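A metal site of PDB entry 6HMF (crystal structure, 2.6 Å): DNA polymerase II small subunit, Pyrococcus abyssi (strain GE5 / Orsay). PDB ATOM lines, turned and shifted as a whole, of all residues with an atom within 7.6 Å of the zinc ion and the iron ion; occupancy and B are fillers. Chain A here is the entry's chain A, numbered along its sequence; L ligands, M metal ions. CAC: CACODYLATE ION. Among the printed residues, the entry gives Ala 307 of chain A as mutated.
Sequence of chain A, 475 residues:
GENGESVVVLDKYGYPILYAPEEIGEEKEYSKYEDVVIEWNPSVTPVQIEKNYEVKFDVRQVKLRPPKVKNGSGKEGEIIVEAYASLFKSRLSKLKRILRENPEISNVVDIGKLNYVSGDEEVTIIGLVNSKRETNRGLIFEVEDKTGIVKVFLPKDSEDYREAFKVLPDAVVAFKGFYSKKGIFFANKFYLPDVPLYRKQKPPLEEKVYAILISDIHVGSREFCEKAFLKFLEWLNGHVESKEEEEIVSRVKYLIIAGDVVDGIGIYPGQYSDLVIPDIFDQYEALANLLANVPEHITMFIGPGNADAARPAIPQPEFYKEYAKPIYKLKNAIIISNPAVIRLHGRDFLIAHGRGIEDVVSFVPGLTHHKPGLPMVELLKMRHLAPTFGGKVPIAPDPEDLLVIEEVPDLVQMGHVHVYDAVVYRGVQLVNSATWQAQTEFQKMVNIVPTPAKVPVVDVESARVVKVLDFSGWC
OD1 of Asp 263 is in hydrogen-bond range of ND1 of His 218 (2.8 Å). The backbone NH (N) of Asp 216 sits at hydrogen-bond distance from the backbone carbonyl oxygen (O) of Gly 259. O of Asp 216 is in hydrogen-bond range of OG1 of Thr 435 (2.7 Å). The side-chain carboxylate (OD1) of Asp 260 sits at hydrogen-bond distance from the backbone NH (N) of Ala 307 (2.8 Å). N of Asp 260 lies within hydrogen-bond range of OD2 of Asp 308, 2.9 Å away. NE2 of His 416 is in hydrogen-bond range of OE1 of Glu 358. ND1 of His 353 is in hydrogen-bond range of O of Ala 258 (2.8 Å). A ring nitrogen (ND1) of His 418 is in hydrogen-bond range of the side-chain amide nitrogen (NE2) of Gln 443 (3.5 Å).
Within 4 Å of the zinc ion: Asp 216, Asp 260, Asn 306, His 353 and His 416. Along chain A the residues within 4 Å of the zinc ion span positions 216 to 416. The nearest printed residue that does not touch the zinc ion is Arg 355 (4.9 Å).
Of the 27 residues printed, 4 come within 4 Å of the iron ion. The nearest printed residue that does not touch the iron ion is His 416 (4.04 Å).
OD2 of Asp 260 binds the zinc ion. OD1 of Asn 306 is bound to the zinc ion. The zinc ion is bound by NE2 of His 353, 2.2 Å away. ND1 of His 416 is bound to the zinc ion, at 2.3 Å. Slightly farther from the zinc ion lies an oxygen (O2) of the ligand (2.8 Å).
O2 of the ligand is bound to the iron ion, 1.8 Å away. The iron ion is bound by OD2 of Asp 216, 2.0 Å away. NE2 of His 218 binds the iron ion (2.2 Å). The iron ion is bound by a ring nitrogen (NE2) of His 418. The iron ion is bound by OD2 of Asp 260, at 2.5 Å. The iron ion has five donor atoms within binding distance.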
ATOM      1  N   SER A 215      -1.968  -8.791 -10.371  1.00  0.00           N
ATOM      2  CA  SER A 215      -2.693  -7.550 -10.635  1.00  0.00           C
ATOM      3  C   SER A 215      -2.482  -7.181 -12.102  1.00  0.00           C
ATOM      4  O   SER A 215      -1.697  -7.837 -12.795  1.00  0.00           O
ATOM      5  CB  SER A 215      -2.221  -6.408  -9.734  1.00  0.00           C
ATOM      6  OG  SER A 215      -0.901  -5.984 -10.031  1.00  0.00           O
ATOM      7  N   ASP A 216      -3.183  -6.127 -12.533  1.00  0.00           N
ATOM      8  CA  ASP A 216      -3.119  -5.506 -13.852  1.00  0.00           C
ATOM      9  C   ASP A 216      -3.086  -6.545 -14.975  1.00  0.00           C
ATOM     10  O   ASP A 216      -2.155  -6.589 -15.782  1.00  0.00           O
ATOM     11  CB  ASP A 216      -1.954  -4.521 -13.909  1.00  0.00           C
ATOM     12  CG  ASP A 216      -2.085  -3.407 -12.891  1.00  0.00           C
ATOM     13  OD1 ASP A 216      -1.768  -3.655 -11.709  1.00  0.00           O
ATOM     14  OD2 ASP A 216      -2.537  -2.320 -13.271  1.00  0.00           O
ATOM     15  N   ILE A 217      -4.116  -7.397 -14.996  1.00  0.00           N
ATOM     16  CA  ILE A 217      -4.284  -8.442 -16.002  1.00  0.00           C
ATOM     17  C   ILE A 217      -4.575  -7.784 -17.362  1.00  0.00           C
ATOM     18  O   ILE A 217      -3.976  -8.170 -18.360  1.00  0.00           O
ATOM     19  CB  ILE A 217      -5.351  -9.483 -15.574  1.00  0.00           C
ATOM     20  CG1 ILE A 217      -5.113  -9.981 -14.114  1.00  0.00           C
ATOM     21  CG2 ILE A 217      -5.364 -10.656 -16.572  1.00  0.00           C
ATOM     22  CD1 ILE A 217      -6.192 -10.890 -13.535  1.00  0.00           C
ATOM     23  N   HIS A 218      -5.432  -6.738 -17.356  1.00  0.00           N
ATOM     24  CA  HIS A 218      -5.809  -5.941 -18.523  1.00  0.00           C
ATOM     25  C   HIS A 218      -6.409  -6.766 -19.653  1.00  0.00           C
ATOM     26  O   HIS A 218      -6.043  -6.565 -20.821  1.00  0.00           O
ATOM     27  CB  HIS A 218      -4.666  -5.044 -19.021  1.00  0.00           C
ATOM     28  CG  HIS A 218      -4.384  -3.897 -18.114  1.00  0.00           C
ATOM     29  ND1 HIS A 218      -5.030  -2.686 -18.252  1.00  0.00           N
ATOM     30  CD2 HIS A 218      -3.576  -3.835 -17.034  1.00  0.00           C
ATOM     31  CE1 HIS A 218      -4.587  -1.916 -17.273  1.00  0.00           C
ATOM     32  NE2 HIS A 218      -3.717  -2.568 -16.515  1.00  0.00           N
ATOM     33  N   ALA A 258      -5.047  -7.383  -7.284  1.00  0.00           N
ATOM     34  CA  ALA A 258      -5.057  -5.960  -6.925  1.00  0.00           C
ATOM     35  C   ALA A 258      -5.328  -4.967  -8.075  1.00  0.00           C
ATOM     36  O   ALA A 258      -4.535  -4.057  -8.309  1.00  0.00           O
ATOM     37  CB  ALA A 258      -3.767  -5.596  -6.205  1.00  0.00           C
ATOM     38  N   GLY A 259      -6.474  -5.119  -8.721  1.00  0.00           N
ATOM     39  CA  GLY A 259      -6.947  -4.172  -9.729  1.00  0.00           C
ATOM     40  C   GLY A 259      -6.513  -4.315 -11.166  1.00  0.00           C
ATOM     41  O   GLY A 259      -5.596  -5.074 -11.484  1.00  0.00           O
ATOM     42  N   ASP A 260      -7.181  -3.526 -12.033  1.00  0.00           N
ATOM     43  CA  ASP A 260      -7.057  -3.469 -13.485  1.00  0.00           C
ATOM     44  C   ASP A 260      -7.132  -4.870 -14.100  1.00  0.00           C
ATOM     45  O   ASP A 260      -6.286  -5.278 -14.908  1.00  0.00           O
ATOM     46  CB  ASP A 260      -5.836  -2.671 -13.930  1.00  0.00           C
ATOM     47  CG  ASP A 260      -5.935  -1.177 -13.673  1.00  0.00           C
ATOM     48  OD1 ASP A 260      -7.054  -0.684 -13.432  1.00  0.00           O
ATOM     49  OD2 ASP A 260      -4.897  -0.504 -13.695  1.00  0.00           O
ATOM     50  N   VAL A 261      -8.170  -5.607 -13.696  1.00  0.00           N
ATOM     51  CA  VAL A 261      -8.445  -6.986 -14.095  1.00  0.00           C
ATOM     52  C   VAL A 261      -8.873  -7.018 -15.570  1.00  0.00           C
ATOM     53  O   VAL A 261      -8.587  -7.987 -16.268  1.00  0.00           O
ATOM     54  CB  VAL A 261      -9.411  -7.715 -13.098  1.00  0.00           C
ATOM     55  CG1 VAL A 261      -8.835  -7.714 -11.687  1.00  0.00           C
ATOM     56  CG2 VAL A 261     -10.811  -7.099 -13.085  1.00  0.00           C
ATOM     57  N   VAL A 262      -9.485  -5.919 -16.051  1.00  0.00           N
ATOM     58  CA  VAL A 262      -9.857  -5.715 -17.456  1.00  0.00           C
ATOM     59  C   VAL A 262      -9.183  -4.407 -17.946  1.00  0.00           C
ATOM     60  O   VAL A 262      -8.809  -3.573 -17.116  1.00  0.00           O
ATOM     61  CB  VAL A 262     -11.401  -5.744 -17.722  1.00  0.00           C
ATOM     62  CG1 VAL A 262     -12.031  -7.055 -17.282  1.00  0.00           C
ATOM     63  CG2 VAL A 262     -12.112  -4.544 -17.112  1.00  0.00           C
ATOM     64  N   ASP A 263      -9.029  -4.216 -19.276  1.00  0.00           N
ATOM     65  CA  ASP A 263      -8.416  -2.987 -19.796  1.00  0.00           C
ATOM     66  C   ASP A 263      -9.382  -1.795 -19.761  1.00  0.00           C
ATOM     67  O   ASP A 263      -8.939  -0.648 -19.743  1.00  0.00           O
ATOM     68  CB  ASP A 263      -7.784  -3.171 -21.199  1.00  0.00           C
ATOM     69  CG  ASP A 263      -6.788  -2.085 -21.568  1.00  0.00           C
ATOM     70  OD1 ASP A 263      -5.836  -1.868 -20.793  1.00  0.00           O
ATOM     71  OD2 ASP A 263      -6.961  -1.457 -22.643  1.00  0.00           O
ATOM     72  N   ILE A 267     -10.668   4.756 -21.151  1.00  0.00           N
ATOM     73  CA  ILE A 267      -9.731   5.085 -20.059  1.00  0.00           C
ATOM     74  C   ILE A 267      -8.794   6.240 -20.479  1.00  0.00           C
ATOM     75  O   ILE A 267      -8.508   7.138 -19.679  1.00  0.00           O
ATOM     76  CB  ILE A 267      -8.990   3.825 -19.529  1.00  0.00           C
ATOM     77  CG1 ILE A 267      -9.976   2.711 -19.065  1.00  0.00           C
ATOM     78  CG2 ILE A 267      -7.972   4.150 -18.413  1.00  0.00           C
ATOM     79  CD1 ILE A 267     -11.075   3.104 -18.030  1.00  0.00           C
ATOM     80  N   GLY A 305      -9.472  -1.676  -9.931  1.00  0.00           N
ATOM     81  CA  GLY A 305      -8.443  -0.706 -10.285  1.00  0.00           C
ATOM     82  C   GLY A 305      -9.075   0.456 -11.027  1.00  0.00           C
ATOM     83  O   GLY A 305     -10.307   0.530 -11.089  1.00  0.00           O
ATOM     84  N   ASN A 306      -8.277   1.356 -11.620  1.00  0.00           N
ATOM     85  CA  ASN A 306      -8.812   2.527 -12.331  1.00  0.00           C
ATOM     86  C   ASN A 306      -9.351   2.227 -13.750  1.00  0.00           C
ATOM     87  O   ASN A 306     -10.082   3.048 -14.305  1.00  0.00           O
ATOM     88  CB  ASN A 306      -7.801   3.686 -12.359  1.00  0.00           C
ATOM     89  CG  ASN A 306      -6.478   3.319 -12.973  1.00  0.00           C
ATOM     90  OD1 ASN A 306      -5.734   2.481 -12.458  1.00  0.00           O
ATOM     91  ND2 ASN A 306      -6.162   3.957 -14.097  1.00  0.00           N
ATOM     92  N   ALA A 307      -9.004   1.053 -14.342  1.00  0.00           N
ATOM     93  CA  ALA A 307      -9.449   0.631 -15.685  1.00  0.00           C
ATOM     94  C   ALA A 307     -10.752  -0.113 -15.585  1.00  0.00           C
ATOM     95  O   ALA A 307     -11.491  -0.217 -16.564  1.00  0.00           O
ATOM     96  CB  ALA A 307      -8.388  -0.248 -16.355  1.00  0.00           C
ATOM     97  N   ASP A 308     -11.043  -0.635 -14.395  1.00  0.00           N
ATOM     98  CA  ASP A 308     -12.224  -1.438 -14.076  1.00  0.00           C
ATOM     99  C   ASP A 308     -13.539  -0.688 -14.071  1.00  0.00           C
ATOM    100  O   ASP A 308     -13.573   0.544 -13.966  1.00  0.00           O
ATOM    101  CB  ASP A 308     -12.020  -2.148 -12.728  1.00  0.00           C
ATOM    102  CG  ASP A 308     -11.050  -3.307 -12.852  1.00  0.00           C
ATOM    103  OD1 ASP A 308     -11.238  -4.141 -13.751  1.00  0.00           O
ATOM    104  OD2 ASP A 308     -10.096  -3.358 -12.071  1.00  0.00           O
ATOM    105  N   HIS A 353      -4.881  -0.675  -5.096  1.00  0.00           N
ATOM    106  CA  HIS A 353      -4.483  -0.703  -6.496  1.00  0.00           C
ATOM    107  C   HIS A 353      -3.130  -0.052  -6.741  1.00  0.00           C
ATOM    108  O   HIS A 353      -2.349  -0.571  -7.533  1.00  0.00           O
ATOM    109  CB  HIS A 353      -5.547  -0.130  -7.430  1.00  0.00           C
ATOM    110  CG  HIS A 353      -5.182  -0.280  -8.868  1.00  0.00           C
ATOM    111  ND1 HIS A 353      -4.831  -1.514  -9.403  1.00  0.00           N
ATOM    112  CD2 HIS A 353      -5.042   0.660  -9.826  1.00  0.00           C
ATOM    113  CE1 HIS A 353      -4.516  -1.272 -10.656  1.00  0.00           C
ATOM    114  NE2 HIS A 353      -4.636   0.020 -10.959  1.00  0.00           N
ATOM    115  N   GLY A 354      -2.842   1.055  -6.070  1.00  0.00           N
ATOM    116  CA  GLY A 354      -1.526   1.689  -6.192  1.00  0.00           C
ATOM    117  C   GLY A 354      -1.490   3.064  -6.795  1.00  0.00           C
ATOM    118  O   GLY A 354      -0.409   3.483  -7.229  1.00  0.00           O
ATOM    119  N   ARG A 355      -2.629   3.780  -6.794  1.00  0.00           N
ATOM    120  CA  ARG A 355      -2.741   5.139  -7.328  1.00  0.00           C
ATOM    121  C   ARG A 355      -1.794   6.119  -6.641  1.00  0.00           C
ATOM    122  O   ARG A 355      -1.290   7.036  -7.290  1.00  0.00           O
ATOM    123  CB  ARG A 355      -4.193   5.657  -7.281  1.00  0.00           C
ATOM    124  CG  ARG A 355      -5.214   4.893  -8.141  1.00  0.00           C
ATOM    125  CD  ARG A 355      -4.897   4.779  -9.642  1.00  0.00           C
ATOM    126  NE  ARG A 355      -4.576   6.072 -10.274  1.00  0.00           N
ATOM    127  CZ  ARG A 355      -5.473   6.916 -10.793  1.00  0.00           C
ATOM    128  NH1 ARG A 355      -6.777   6.615 -10.749  1.00  0.00           N
ATOM    129  NH2 ARG A 355      -5.085   8.060 -11.331  1.00  0.00           N
ATOM    130  N   GLU A 358       1.966   6.885  -7.968  1.00  0.00           N
ATOM    131  CA  GLU A 358       2.062   7.967  -8.941  1.00  0.00           C
ATOM    132  C   GLU A 358       2.277   9.311  -8.270  1.00  0.00           C
ATOM    133  O   GLU A 358       3.104  10.084  -8.755  1.00  0.00           O
ATOM    134  CB  GLU A 358       0.791   8.049  -9.794  1.00  0.00           C
ATOM    135  CG  GLU A 358       0.882   7.250 -11.077  1.00  0.00           C
ATOM    136  CD  GLU A 358      -0.222   7.531 -12.063  1.00  0.00           C
ATOM    137  OE1 GLU A 358      -1.412   7.550 -11.666  1.00  0.00           O
ATOM    138  OE2 GLU A 358       0.110   7.665 -13.262  1.00  0.00           O
ATOM    139  N   GLY A 415      -0.603  -2.685  -7.211  1.00  0.00           N
ATOM    140  CA  GLY A 415      -0.432  -2.906  -8.634  1.00  0.00           C
ATOM    141  C   GLY A 415      -0.205  -1.560  -9.288  1.00  0.00           C
ATOM    142  O   GLY A 415       0.645  -0.778  -8.847  1.00  0.00           O
ATOM    143  N   HIS A 416      -1.006  -1.252 -10.315  1.00  0.00           N
ATOM    144  CA  HIS A 416      -1.078   0.010 -11.051  1.00  0.00           C
ATOM    145  C   HIS A 416       0.164   0.400 -11.872  1.00  0.00           C
ATOM    146  O   HIS A 416      -0.002   0.718 -13.040  1.00  0.00           O
ATOM    147  CB  HIS A 416      -1.483   1.173 -10.110  1.00  0.00           C
ATOM    148  CG  HIS A 416      -1.691   2.478 -10.808  1.00  0.00           C
ATOM    149  ND1 HIS A 416      -2.653   2.619 -11.801  1.00  0.00           N
ATOM    150  CD2 HIS A 416      -1.068   3.651 -10.647  1.00  0.00           C
ATOM    151  CE1 HIS A 416      -2.560   3.870 -12.224  1.00  0.00           C
ATOM    152  NE2 HIS A 416      -1.621   4.526 -11.551  1.00  0.00           N
ATOM    153  N   VAL A 417       1.380   0.421 -11.296  1.00  0.00           N
ATOM    154  CA  VAL A 417       2.580   0.892 -12.024  1.00  0.00           C
ATOM    155  C   VAL A 417       3.166  -0.111 -13.046  1.00  0.00           C
ATOM    156  O   VAL A 417       4.032   0.292 -13.865  1.00  0.00           O
ATOM    157  CB  VAL A 417       3.685   1.453 -11.103  1.00  0.00           C
ATOM    158  CG1 VAL A 417       3.147   2.576 -10.239  1.00  0.00           C
ATOM    159  CG2 VAL A 417       4.331   0.349 -10.264  1.00  0.00           C
ATOM    160  N   HIS A 418       2.747  -1.393 -13.001  1.00  0.00           N
ATOM    161  CA  HIS A 418       3.145  -2.451 -13.952  1.00  0.00           C
ATOM    162  C   HIS A 418       4.601  -2.900 -13.841  1.00  0.00           C
ATOM    163  O   HIS A 418       5.091  -3.576 -14.742  1.00  0.00           O
ATOM    164  CB  HIS A 418       2.828  -2.024 -15.404  1.00  0.00           C
ATOM    165  CG  HIS A 418       1.366  -1.973 -15.719  1.00  0.00           C
ATOM    166  ND1 HIS A 418       0.915  -2.008 -17.012  1.00  0.00           N
ATOM    167  CD2 HIS A 418       0.292  -1.903 -14.878  1.00  0.00           C
ATOM    168  CE1 HIS A 418      -0.400  -1.946 -16.943  1.00  0.00           C
ATOM    169  NE2 HIS A 418      -0.818  -1.886 -15.681  1.00  0.00           N
ATOM    170  N   ALA A 434       3.143  -6.366 -10.267  1.00  0.00           N
ATOM    171  CA  ALA A 434       3.397  -6.071 -11.678  1.00  0.00           C
ATOM    172  C   ALA A 434       2.137  -6.061 -12.569  1.00  0.00           C
ATOM    173  O   ALA A 434       1.175  -5.351 -12.251  1.00  0.00           O
ATOM    174  CB  ALA A 434       4.462  -7.011 -12.249  1.00  0.00           C
ATOM    175  N   THR A 435       2.182  -6.788 -13.720  1.00  0.00           N
ATOM    176  CA  THR A 435       1.132  -6.805 -14.740  1.00  0.00           C
ATOM    177  C   THR A 435       1.205  -8.036 -15.645  1.00  0.00           C
ATOM    178  O   THR A 435       2.230  -8.730 -15.689  1.00  0.00           O
ATOM    179  CB  THR A 435       1.273  -5.522 -15.619  1.00  0.00           C
ATOM    180  OG1 THR A 435       0.164  -5.397 -16.501  1.00  0.00           O
ATOM    181  CG2 THR A 435       2.596  -5.467 -16.419  1.00  0.00           C
ATOM    182  N   GLN A 437       0.236  -7.317 -18.850  1.00  0.00           N
ATOM    183  CA  GLN A 437       0.147  -6.486 -20.030  1.00  0.00           C
ATOM    184  C   GLN A 437       1.519  -6.000 -20.472  1.00  0.00           C
ATOM    185  O   GLN A 437       2.209  -5.341 -19.696  1.00  0.00           O
ATOM    186  CB  GLN A 437      -0.791  -5.292 -19.786  1.00  0.00           C
ATOM    187  CG  GLN A 437      -0.915  -4.344 -20.982  1.00  0.00           C
ATOM    188  CD  GLN A 437      -1.812  -3.163 -20.748  1.00  0.00           C
ATOM    189  OE1 GLN A 437      -1.599  -2.327 -19.852  1.00  0.00           O
ATOM    190  NE2 GLN A 437      -2.793  -3.016 -21.609  1.00  0.00           N
ATOM    191  N   GLN A 443       1.943   3.624 -23.239  1.00  0.00           N
ATOM    192  CA  GLN A 443       2.969   3.417 -22.214  1.00  0.00           C
ATOM    193  C   GLN A 443       4.352   3.854 -22.743  1.00  0.00           C
ATOM    194  O   GLN A 443       5.079   4.552 -22.045  1.00  0.00           O
ATOM    195  CB  GLN A 443       2.981   1.964 -21.723  1.00  0.00           C
ATOM    196  CG  GLN A 443       1.813   1.627 -20.787  1.00  0.00           C
ATOM    197  CD  GLN A 443       1.501   0.143 -20.632  1.00  0.00           C
ATOM    198  OE1 GLN A 443       2.200  -0.727 -21.137  1.00  0.00           O
ATOM    199  NE2 GLN A 443       0.454  -0.165 -19.908  1.00  0.00           N
HETATM  200 AS   CAC L   1      -2.907   1.745 -15.985  1.00  0.00          AS
HETATM  201  O1  CAC L   1      -4.170   2.767 -15.653  1.00  0.00           O
HETATM  202  O2  CAC L   1      -2.610   0.360 -15.112  1.00  0.00           O
HETATM  203  C1  CAC L   1      -2.953   1.294 -17.906  1.00  0.00           C
HETATM  204  C2  CAC L   1      -1.220   2.785 -16.011  1.00  0.00           C
HETATM  205 ZN    ZN M   1      -4.073   1.157 -12.815  1.00  0.00          ZN
HETATM  206 FE    FE M   2      -2.921  -1.353 -14.924  1.00  0.00          FE
